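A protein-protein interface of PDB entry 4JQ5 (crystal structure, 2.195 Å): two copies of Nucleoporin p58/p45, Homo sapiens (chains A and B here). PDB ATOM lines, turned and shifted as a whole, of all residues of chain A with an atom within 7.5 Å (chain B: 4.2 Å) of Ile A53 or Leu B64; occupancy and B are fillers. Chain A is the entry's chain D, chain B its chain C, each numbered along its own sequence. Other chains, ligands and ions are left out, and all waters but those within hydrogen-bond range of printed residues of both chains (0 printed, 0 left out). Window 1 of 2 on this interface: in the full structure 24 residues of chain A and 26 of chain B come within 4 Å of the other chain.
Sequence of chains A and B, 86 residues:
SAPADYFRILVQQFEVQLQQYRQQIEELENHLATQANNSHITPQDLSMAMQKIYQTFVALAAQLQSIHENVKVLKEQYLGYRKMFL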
ATOM      1  N   TYR A  21      29.378  10.349  -5.806  1.00  0.00           N
ATOM      2  CA  TYR A  21      28.947  10.937  -4.547  1.00  0.00           C
ATOM      3  C   TYR A  21      28.682  12.423  -4.727  1.00  0.00           C
ATOM      4  O   TYR A  21      27.616  12.927  -4.363  1.00  0.00           O
ATOM      5  CB  TYR A  21      30.034  10.719  -3.498  1.00  0.00           C
ATOM      6  CG  TYR A  21      29.679  11.167  -2.099  1.00  0.00           C
ATOM      7  CD1 TYR A  21      28.614  10.600  -1.415  1.00  0.00           C
ATOM      8  CD2 TYR A  21      30.432  12.134  -1.450  1.00  0.00           C
ATOM      9  CE1 TYR A  21      28.298  10.998  -0.131  1.00  0.00           C
ATOM     10  CE2 TYR A  21      30.125  12.538  -0.167  1.00  0.00           C
ATOM     11  CZ  TYR A  21      29.058  11.967   0.488  1.00  0.00           C
ATOM     12  OH  TYR A  21      28.754  12.367   1.768  1.00  0.00           O
ATOM     13  N   GLN A  24      25.471  13.083  -6.626  1.00  0.00           N
ATOM     14  CA  GLN A  24      24.247  12.911  -5.849  1.00  0.00           C
ATOM     15  C   GLN A  24      24.004  14.120  -4.949  1.00  0.00           C
ATOM     16  O   GLN A  24      22.872  14.593  -4.823  1.00  0.00           O
ATOM     17  CB  GLN A  24      24.312  11.627  -5.020  1.00  0.00           C
ATOM     18  CG  GLN A  24      24.033  10.367  -5.829  1.00  0.00           C
ATOM     19  CD  GLN A  24      24.373   9.096  -5.075  1.00  0.00           C
ATOM     20  OE1 GLN A  24      25.326   9.059  -4.294  1.00  0.00           O
ATOM     21  NE2 GLN A  24      23.595   8.045  -5.304  1.00  0.00           N
ATOM     22  N   ILE A  25      25.069  14.623  -4.334  1.00  0.00           N
ATOM     23  CA  ILE A  25      24.968  15.795  -3.472  1.00  0.00           C
ATOM     24  C   ILE A  25      24.646  17.055  -4.272  1.00  0.00           C
ATOM     25  O   ILE A  25      23.929  17.931  -3.790  1.00  0.00           O
ATOM     26  CB  ILE A  25      26.268  16.030  -2.689  1.00  0.00           C
ATOM     27  CG1 ILE A  25      26.511  14.871  -1.722  1.00  0.00           C
ATOM     28  CG2 ILE A  25      26.199  17.349  -1.926  1.00  0.00           C
ATOM     29  CD1 ILE A  25      27.842  14.940  -1.026  1.00  0.00           C
ATOM     30  N   GLU A  26      25.182  17.141  -5.486  1.00  0.00           N
ATOM     31  CA  GLU A  26      24.961  18.300  -6.345  1.00  0.00           C
ATOM     32  C   GLU A  26      23.516  18.317  -6.819  1.00  0.00           C
ATOM     33  O   GLU A  26      22.881  19.368  -6.876  1.00  0.00           O
ATOM     34  CB  GLU A  26      25.902  18.271  -7.554  1.00  0.00           C
ATOM     35  CG  GLU A  26      27.325  18.720  -7.255  1.00  0.00           C
ATOM     36  CD  GLU A  26      28.238  18.628  -8.467  1.00  0.00           C
ATOM     37  OE1 GLU A  26      27.801  18.090  -9.507  1.00  0.00           O
ATOM     38  OE2 GLU A  26      29.393  19.097  -8.381  1.00  0.00           O
ATOM     39  N   LEU A  28      20.919  16.931  -5.284  1.00  0.00           N
ATOM     40  CA  LEU A  28      20.139  17.321  -4.118  1.00  0.00           C
ATOM     41  C   LEU A  28      20.303  18.815  -3.840  1.00  0.00           C
ATOM     42  O   LEU A  28      19.366  19.481  -3.405  1.00  0.00           O
ATOM     43  CB  LEU A  28      20.576  16.492  -2.905  1.00  0.00           C
ATOM     44  CG  LEU A  28      19.865  16.711  -1.565  1.00  0.00           C
ATOM     45  CD1 LEU A  28      20.481  17.875  -0.803  1.00  0.00           C
ATOM     46  CD2 LEU A  28      18.368  16.923  -1.764  1.00  0.00           C
ATOM     47  N   GLU A  29      21.494  19.338  -4.113  1.00  0.00           N
ATOM     48  CA  GLU A  29      21.800  20.739  -3.848  1.00  0.00           C
ATOM     49  C   GLU A  29      21.107  21.656  -4.856  1.00  0.00           C
ATOM     50  O   GLU A  29      20.812  22.814  -4.554  1.00  0.00           O
ATOM     51  CB  GLU A  29      23.313  20.962  -3.882  1.00  0.00           C
ATOM     52  CG  GLU A  29      23.752  22.348  -3.435  1.00  0.00           C
ATOM     53  CD  GLU A  29      25.253  22.443  -3.234  1.00  0.00           C
ATOM     54  OE1 GLU A  29      25.918  21.387  -3.205  1.00  0.00           O
ATOM     55  OE2 GLU A  29      25.771  23.573  -3.105  1.00  0.00           O
ATOM     56  N   LEU A  46      13.764  20.041   4.215  1.00  0.00           N
ATOM     57  CA  LEU A  46      15.025  20.009   4.948  1.00  0.00           C
ATOM     58  C   LEU A  46      15.254  18.643   5.589  1.00  0.00           C
ATOM     59  O   LEU A  46      16.371  18.118   5.580  1.00  0.00           O
ATOM     60  CB  LEU A  46      15.046  21.091   6.028  1.00  0.00           C
ATOM     61  CG  LEU A  46      16.330  21.921   6.096  1.00  0.00           C
ATOM     62  CD1 LEU A  46      16.235  22.926   7.227  1.00  0.00           C
ATOM     63  CD2 LEU A  46      17.558  21.035   6.266  1.00  0.00           C
ATOM     64  N   SER A  47      14.190  18.071   6.143  1.00  0.00           N
ATOM     65  CA  SER A  47      14.278  16.774   6.801  1.00  0.00           C
ATOM     66  C   SER A  47      14.683  15.669   5.823  1.00  0.00           C
ATOM     67  O   SER A  47      15.649  14.946   6.061  1.00  0.00           O
ATOM     68  CB  SER A  47      12.945  16.421   7.459  1.00  0.00           C
ATOM     69  OG  SER A  47      12.999  15.132   8.042  1.00  0.00           O
ATOM     70  N   MET A  48      13.934  15.541   4.729  1.00  0.00           N
ATOM     71  CA  MET A  48      14.199  14.514   3.721  1.00  0.00           C
ATOM     72  C   MET A  48      15.588  14.685   3.094  1.00  0.00           C
ATOM     73  O   MET A  48      16.234  13.710   2.686  1.00  0.00           O
ATOM     74  CB  MET A  48      13.132  14.567   2.625  1.00  0.00           C
ATOM     75  CG  MET A  48      11.737  14.161   3.081  1.00  0.00           C
ATOM     76  SD  MET A  48      10.491  14.363   1.790  1.00  0.00           S
ATOM     77  CE  MET A  48      11.119  13.263   0.522  1.00  0.00           C
ATOM     78  N   ALA A  49      16.042  15.932   3.028  1.00  0.00           N
ATOM     79  CA  ALA A  49      17.326  16.256   2.417  1.00  0.00           C
ATOM     80  C   ALA A  49      18.449  15.722   3.295  1.00  0.00           C
ATOM     81  O   ALA A  49      19.378  15.069   2.810  1.00  0.00           O
ATOM     82  CB  ALA A  49      17.462  17.761   2.240  1.00  0.00           C
ATOM     83  N   MET A  50      18.350  15.999   4.591  1.00  0.00           N
ATOM     84  CA  MET A  50      19.335  15.520   5.549  1.00  0.00           C
ATOM     85  C   MET A  50      19.364  14.001   5.502  1.00  0.00           C
ATOM     86  O   MET A  50      20.429  13.395   5.495  1.00  0.00           O
ATOM     87  CB  MET A  50      19.001  16.001   6.964  1.00  0.00           C
ATOM     88  CG  MET A  50      19.202  17.494   7.182  1.00  0.00           C
ATOM     89  SD  MET A  50      19.151  17.980   8.920  1.00  0.00           S
ATOM     90  CE  MET A  50      17.649  17.172   9.470  1.00  0.00           C
ATOM     91  N   GLN A  51      18.182  13.396   5.453  1.00  0.00           N
ATOM     92  CA  GLN A  51      18.062  11.946   5.384  1.00  0.00           C
ATOM     93  C   GLN A  51      18.770  11.422   4.136  1.00  0.00           C
ATOM     94  O   GLN A  51      19.361  10.341   4.148  1.00  0.00           O
ATOM     95  CB  GLN A  51      16.589  11.537   5.371  1.00  0.00           C
ATOM     96  CG  GLN A  51      16.359  10.049   5.159  1.00  0.00           C
ATOM     97  CD  GLN A  51      14.893   9.664   5.249  1.00  0.00           C
ATOM     98  OE1 GLN A  51      14.128  10.263   6.006  1.00  0.00           O
ATOM     99  NE2 GLN A  51      14.494   8.662   4.473  1.00  0.00           N
ATOM    100  N   LYS A  52      18.703  12.199   3.059  1.00  0.00           N
ATOM    101  CA  LYS A  52      19.364  11.828   1.809  1.00  0.00           C
ATOM    102  C   LYS A  52      20.880  11.900   1.954  1.00  0.00           C
ATOM    103  O   LYS A  52      21.608  11.077   1.393  1.00  0.00           O
ATOM    104  CB  LYS A  52      18.908  12.747   0.673  1.00  0.00           C
ATOM    105  CG  LYS A  52      18.353  12.014  -0.542  1.00  0.00           C
ATOM    106  CD  LYS A  52      19.457  11.511  -1.461  1.00  0.00           C
ATOM    107  CE  LYS A  52      18.883  10.862  -2.714  1.00  0.00           C
ATOM    108  NZ  LYS A  52      19.928  10.593  -3.742  1.00  0.00           N
ATOM    109  N   ILE A  53      21.348  12.890   2.707  1.00  0.00           N
ATOM    110  CA  ILE A  53      22.773  13.052   2.953  1.00  0.00           C
ATOM    111  C   ILE A  53      23.325  11.863   3.740  1.00  0.00           C
ATOM    112  O   ILE A  53      24.317  11.263   3.340  1.00  0.00           O
ATOM    113  CB  ILE A  53      23.075  14.362   3.710  1.00  0.00           C
ATOM    114  CG1 ILE A  53      22.682  15.573   2.861  1.00  0.00           C
ATOM    115  CG2 ILE A  53      24.552  14.439   4.078  1.00  0.00           C
ATOM    116  CD1 ILE A  53      23.478  15.710   1.581  1.00  0.00           C
ATOM    117  N   TYR A  54      22.681  11.516   4.851  1.00  0.00           N
ATOM    118  CA  TYR A  54      23.140  10.402   5.677  1.00  0.00           C
ATOM    119  C   TYR A  54      23.106   9.089   4.899  1.00  0.00           C
ATOM    120  O   TYR A  54      24.036   8.284   4.973  1.00  0.00           O
ATOM    121  CB  TYR A  54      22.285  10.277   6.941  1.00  0.00           C
ATOM    122  CG  TYR A  54      22.641  11.269   8.030  1.00  0.00           C
ATOM    123  CD1 TYR A  54      23.674  11.011   8.920  1.00  0.00           C
ATOM    124  CD2 TYR A  54      21.938  12.458   8.169  1.00  0.00           C
ATOM    125  CE1 TYR A  54      24.001  11.914   9.918  1.00  0.00           C
ATOM    126  CE2 TYR A  54      22.257  13.366   9.162  1.00  0.00           C
ATOM    127  CZ  TYR A  54      23.289  13.089  10.033  1.00  0.00           C
ATOM    128  OH  TYR A  54      23.610  13.989  11.024  1.00  0.00           O
ATOM    129  N   GLN A  55      22.025   8.881   4.152  1.00  0.00           N
ATOM    130  CA  GLN A  55      21.829   7.651   3.395  1.00  0.00           C
ATOM    131  C   GLN A  55      22.876   7.503   2.299  1.00  0.00           C
ATOM    132  O   GLN A  55      23.381   6.409   2.049  1.00  0.00           O
ATOM    133  CB  GLN A  55      20.433   7.642   2.768  1.00  0.00           C
ATOM    134  CG  GLN A  55      20.170   6.454   1.848  1.00  0.00           C
ATOM    135  CD  GLN A  55      18.794   6.488   1.207  1.00  0.00           C
ATOM    136  OE1 GLN A  55      17.981   7.371   1.490  1.00  0.00           O
ATOM    137  NE2 GLN A  55      18.527   5.520   0.336  1.00  0.00           N
ATOM    138  N   THR A  56      23.196   8.613   1.646  1.00  0.00           N
ATOM    139  CA  THR A  56      24.097   8.584   0.505  1.00  0.00           C
ATOM    140  C   THR A  56      25.520   8.414   1.010  1.00  0.00           C
ATOM    141  O   THR A  56      26.337   7.766   0.362  1.00  0.00           O
ATOM    142  CB  THR A  56      23.967   9.857  -0.371  1.00  0.00           C
ATOM    143  OG1 THR A  56      24.664   9.672  -1.611  1.00  0.00           O
ATOM    144  CG2 THR A  56      24.510  11.089   0.347  1.00  0.00           C
ATOM    145  N   PHE A  57      25.807   8.974   2.185  1.00  0.00           N
ATOM    146  CA  PHE A  57      27.125   8.811   2.785  1.00  0.00           C
ATOM    147  C   PHE A  57      27.359   7.394   3.290  1.00  0.00           C
ATOM    148  O   PHE A  57      28.480   6.899   3.228  1.00  0.00           O
ATOM    149  CB  PHE A  57      27.393   9.789   3.934  1.00  0.00           C
ATOM    150  CG  PHE A  57      28.693   9.506   4.646  1.00  0.00           C
ATOM    151  CD1 PHE A  57      29.903   9.902   4.093  1.00  0.00           C
ATOM    152  CD2 PHE A  57      28.711   8.790   5.833  1.00  0.00           C
ATOM    153  CE1 PHE A  57      31.103   9.619   4.729  1.00  0.00           C
ATOM    154  CE2 PHE A  57      29.909   8.503   6.472  1.00  0.00           C
ATOM    155  CZ  PHE A  57      31.104   8.919   5.918  1.00  0.00           C
ATOM    156  N   VAL A  58      26.322   6.748   3.813  1.00  0.00           N
ATOM    157  CA  VAL A  58      26.466   5.371   4.275  1.00  0.00           C
ATOM    158  C   VAL A  58      26.822   4.463   3.099  1.00  0.00           C
ATOM    159  O   VAL A  58      27.612   3.531   3.241  1.00  0.00           O
ATOM    160  CB  VAL A  58      25.190   4.864   4.968  1.00  0.00           C
ATOM    161  CG1 VAL A  58      25.232   3.347   5.155  1.00  0.00           C
ATOM    162  CG2 VAL A  58      25.021   5.559   6.310  1.00  0.00           C
ATOM    163  N   ALA A  59      26.247   4.755   1.935  1.00  0.00           N
ATOM    164  CA  ALA A  59      26.548   4.010   0.719  1.00  0.00           C
ATOM    165  C   ALA A  59      27.989   4.267   0.299  1.00  0.00           C
ATOM    166  O   ALA A  59      28.737   3.332   0.008  1.00  0.00           O
ATOM    167  CB  ALA A  59      25.585   4.401  -0.399  1.00  0.00           C
ATOM    168  N   PHE B  14      21.912  25.471   5.796  1.00  0.00           N
ATOM    169  CA  PHE B  14      22.012  24.105   5.303  1.00  0.00           C
ATOM    170  C   PHE B  14      22.649  24.071   3.916  1.00  0.00           C
ATOM    171  O   PHE B  14      23.639  23.374   3.696  1.00  0.00           O
ATOM    172  CB  PHE B  14      20.634  23.449   5.251  1.00  0.00           C
ATOM    173  CG  PHE B  14      20.643  22.079   4.639  1.00  0.00           C
ATOM    174  CD1 PHE B  14      20.888  20.960   5.416  1.00  0.00           C
ATOM    175  CD2 PHE B  14      20.415  21.910   3.283  1.00  0.00           C
ATOM    176  CE1 PHE B  14      20.902  19.697   4.853  1.00  0.00           C
ATOM    177  CE2 PHE B  14      20.426  20.650   2.717  1.00  0.00           C
ATOM    178  CZ  PHE B  14      20.670  19.542   3.503  1.00  0.00           C
ATOM    179  N   LEU B  18      26.367  22.661   2.780  1.00  0.00           N
ATOM    180  CA  LEU B  18      26.445  21.599   1.792  1.00  0.00           C
ATOM    181  C   LEU B  18      27.365  22.029   0.653  1.00  0.00           C
ATOM    182  O   LEU B  18      28.068  21.210   0.062  1.00  0.00           O
ATOM    183  CB  LEU B  18      25.042  21.288   1.269  1.00  0.00           C
ATOM    184  CG  LEU B  18      24.745  19.868   0.789  1.00  0.00           C
ATOM    185  CD1 LEU B  18      25.350  18.821   1.711  1.00  0.00           C
ATOM    186  CD2 LEU B  18      23.240  19.676   0.695  1.00  0.00           C
ATOM    187  N   LEU B  60      30.453  17.838   8.753  1.00  0.00           N
ATOM    188  CA  LEU B  60      29.180  18.138   8.109  1.00  0.00           C
ATOM    189  C   LEU B  60      28.009  17.669   8.962  1.00  0.00           C
ATOM    190  O   LEU B  60      26.988  18.347   9.047  1.00  0.00           O
ATOM    191  CB  LEU B  60      29.100  17.479   6.733  1.00  0.00           C
ATOM    192  CG  LEU B  60      27.718  17.540   6.077  1.00  0.00           C
ATOM    193  CD1 LEU B  60      27.317  18.985   5.802  1.00  0.00           C
ATOM    194  CD2 LEU B  60      27.685  16.721   4.801  1.00  0.00           C
ATOM    195  N   ALA B  61      28.168  16.517   9.607  1.00  0.00           N
ATOM    196  CA  ALA B  61      27.075  15.886  10.333  1.00  0.00           C
ATOM    197  C   ALA B  61      26.804  16.656  11.614  1.00  0.00           C
ATOM    198  O   ALA B  61      25.662  16.759  12.054  1.00  0.00           O
ATOM    199  CB  ALA B  61      27.403  14.438  10.644  1.00  0.00           C
ATOM    200  N   ALA B  62      27.864  17.182  12.219  1.00  0.00           N
ATOM    201  CA  ALA B  62      27.714  18.061  13.370  1.00  0.00           C
ATOM    202  C   ALA B  62      26.906  19.293  12.974  1.00  0.00           C
ATOM    203  O   ALA B  62      26.007  19.712  13.701  1.00  0.00           O
ATOM    204  CB  ALA B  62      29.074  18.465  13.911  1.00  0.00           C
ATOM    205  N   GLN B  63      27.226  19.874  11.821  1.00  0.00           N
ATOM    206  CA  GLN B  63      26.466  21.018  11.316  1.00  0.00           C
ATOM    207  C   GLN B  63      24.986  20.666  11.116  1.00  0.00           C
ATOM    208  O   GLN B  63      24.091  21.440  11.482  1.00  0.00           O
ATOM    209  CB  GLN B  63      27.059  21.516   9.997  1.00  0.00           C
ATOM    210  CG  GLN B  63      28.502  21.995  10.095  1.00  0.00           C
ATOM    211  CD  GLN B  63      28.634  23.314  10.828  1.00  0.00           C
ATOM    212  OE1 GLN B  63      27.674  24.075  10.939  1.00  0.00           O
ATOM    213  NE2 GLN B  63      29.831  23.591  11.335  1.00  0.00           N
ATOM    214  N   LEU B  64      24.734  19.494  10.538  1.00  0.00           N
ATOM    215  CA  LEU B  64      23.375  19.068  10.221  1.00  0.00           C
ATOM    216  C   LEU B  64      22.557  18.822  11.482  1.00  0.00           C
ATOM    217  O   LEU B  64      21.358  19.100  11.517  1.00  0.00           O
ATOM    218  CB  LEU B  64      23.391  17.797   9.368  1.00  0.00           C
ATOM    219  CG  LEU B  64      23.992  17.906   7.964  1.00  0.00           C
ATOM    220  CD1 LEU B  64      23.714  16.637   7.173  1.00  0.00           C
ATOM    221  CD2 LEU B  64      23.466  19.125   7.230  1.00  0.00           C
ATOM    222  N   GLN B  65      23.204  18.296  12.515  1.00  0.00           N
ATOM    223  CA  GLN B  65      22.516  18.010  13.766  1.00  0.00           C
ATOM    224  C   GLN B  65      22.209  19.328  14.462  1.00  0.00           C
ATOM    225  O   GLN B  65      21.169  19.481  15.099  1.00  0.00           O
ATOM    226  CB  GLN B  65      23.371  17.114  14.665  1.00  0.00           C
ATOM    227  CG  GLN B  65      22.581  16.026  15.377  1.00  0.00           C
ATOM    228  CD  GLN B  65      21.897  15.072  14.411  1.00  0.00           C
ATOM    229  OE1 GLN B  65      22.111  15.137  13.200  1.00  0.00           O
ATOM    230  NE2 GLN B  65      21.068  14.181  14.944  1.00  0.00           N
ATOM    231  N   SER B  66      23.121  20.284  14.326  1.00  0.00           N
ATOM    232  CA  SER B  66      22.917  21.614  14.876  1.00  0.00           C
ATOM    233  C   SER B  66      21.641  22.232  14.311  1.00  0.00           C
ATOM    234  O   SER B  66      20.779  22.683  15.067  1.00  0.00           O
ATOM    235  CB  SER B  66      24.123  22.505  14.570  1.00  0.00           C
ATOM    236  OG  SER B  66      23.938  23.810  15.089  1.00  0.00           O
ATOM    237  N   ILE B  67      21.511  22.247  12.987  1.00  0.00           N
ATOM    238  CA  ILE B  67      20.312  22.821  12.374  1.00  0.00           C
ATOM    239  C   ILE B  67      19.075  21.963  12.667  1.00  0.00           C
ATOM    240  O   ILE B  67      17.954  22.476  12.760  1.00  0.00           O
ATOM    241  CB  ILE B  67      20.466  23.028  10.846  1.00  0.00           C
ATOM    242  CG1 ILE B  67      20.289  21.711  10.093  1.00  0.00           C
ATOM    243  CG2 ILE B  67      21.802  23.690  10.512  1.00  0.00           C
ATOM    244  CD1 ILE B  67      18.914  21.549   9.479  1.00  0.00           C
ATOM    245  N   HIS B  68      19.283  20.657  12.826  1.00  0.00           N
ATOM    246  CA  HIS B  68      18.189  19.740  13.127  1.00  0.00           C
ATOM    247  C   HIS B  68      17.561  20.058  14.482  1.00  0.00           C
ATOM    248  O   HIS B  68      16.348  19.935  14.660  1.00  0.00           O
ATOM    249  CB  HIS B  68      18.680  18.293  13.117  1.00  0.00           C
ATOM    250  CG  HIS B  68      17.675  17.311  13.638  1.00  0.00           C
ATOM    251  ND1 HIS B  68      16.463  17.087  13.022  1.00  0.00           N
ATOM    252  CD2 HIS B  68      17.705  16.496  14.719  1.00  0.00           C
ATOM    253  CE1 HIS B  68      15.788  16.175  13.701  1.00  0.00           C
ATOM    254  NE2 HIS B  68      16.520  15.801  14.734  1.00  0.00           N
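The side-chain sulfur (SD) of Met A50 sits close to the backbone carbonyl oxygen (O) of Leu B64 (3.6 Å). The side-chain amide oxygen (OE1) of Gln B65 is in hydrogen-bond range of the side-chain hydroxyl (OH) of Tyr A54 (2.9 Å).
CG2 of Ile A25 touches CG of Leu B18, 3.98 Å away. Phe B14 touches Leu A46 (CD1 to CD2, 3.4 Å). CD1 of Ile B67 touches CD2 of Leu A46, at 3.5 Å. Ala A49 touches Phe B14 (CB to CZ, 3.9 Å). CG of Met A50 touches CE1 of Phe B14, at 3.6 Å. Met A50 touches Ile B67 (SD to CD1, 3.6 Å). His B68 touches Met A50. Ile A53 touches Leu B60 (CG2 to CD2, 3.9 Å). CG2 of Ile A53 touches CD1 of Leu B64 (3.9 Å). Ala B61 touches Tyr A54.
Ile A53 touches just these residues of chain B: Leu B18 (3.6 Å), Leu B60 (3.9 Å) and Leu B64 (3.9 Å). Of chain A, only Met A50 (3.6 Å) and Ile A53 (3.9 Å) come within 4 Å of Leu B64. Printed residues of chain A within 4 Å of Leu B60: Ile A53. Of the printed residues of chain A, Ile B67 touches Leu A46 and Met A50. Printed residues of chain B within 4 Å of Leu A46: Phe B14 (3.4 Å) and Ile B67 (3.5 Å). Printed residues of chain B within 4 Å of Met A50: Phe B14, Leu B64, Ile B67 and His B68. Printed residues of chain B within 4 Å of Tyr A54: Ala B61 and Gln B65. Lys A52 touches none of the printed residues of chain B. Gln A51 touches none of the printed residues of chain B. The nearest residue of chain A that does not touch Leu B64 is Tyr A54 (4.1 Å). The nearest printed residue of chain B that does not touch Leu A28 is Phe B14 (4.5 Å).
Of the 20 printed residues of chain A, 8 touch a printed residue of chain B. Hydrophobic or aromatic side chains of chain A within 4 Å of the printed part of chain B: Ile A25, Leu A28, Leu A46, Ala A49, Met A50, Ile A53 and Tyr A54. Printed residues of chain B that touch a printed residue of chain A: Phe B14, Leu B18, Leu B60, Ala B61, Leu B64, Gln B65, Ile B67 and His B68. Hydrophobic or aromatic side chains of chain B within 4 Å of the printed part of chain A: Phe B14, Leu B18, Leu B60, Ala B61, Leu B64, Ile B67 and His B68. Along chain B the printed residues that touch a printed residue of chain A span positions 14 to 68.
No position is printed for both chains.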
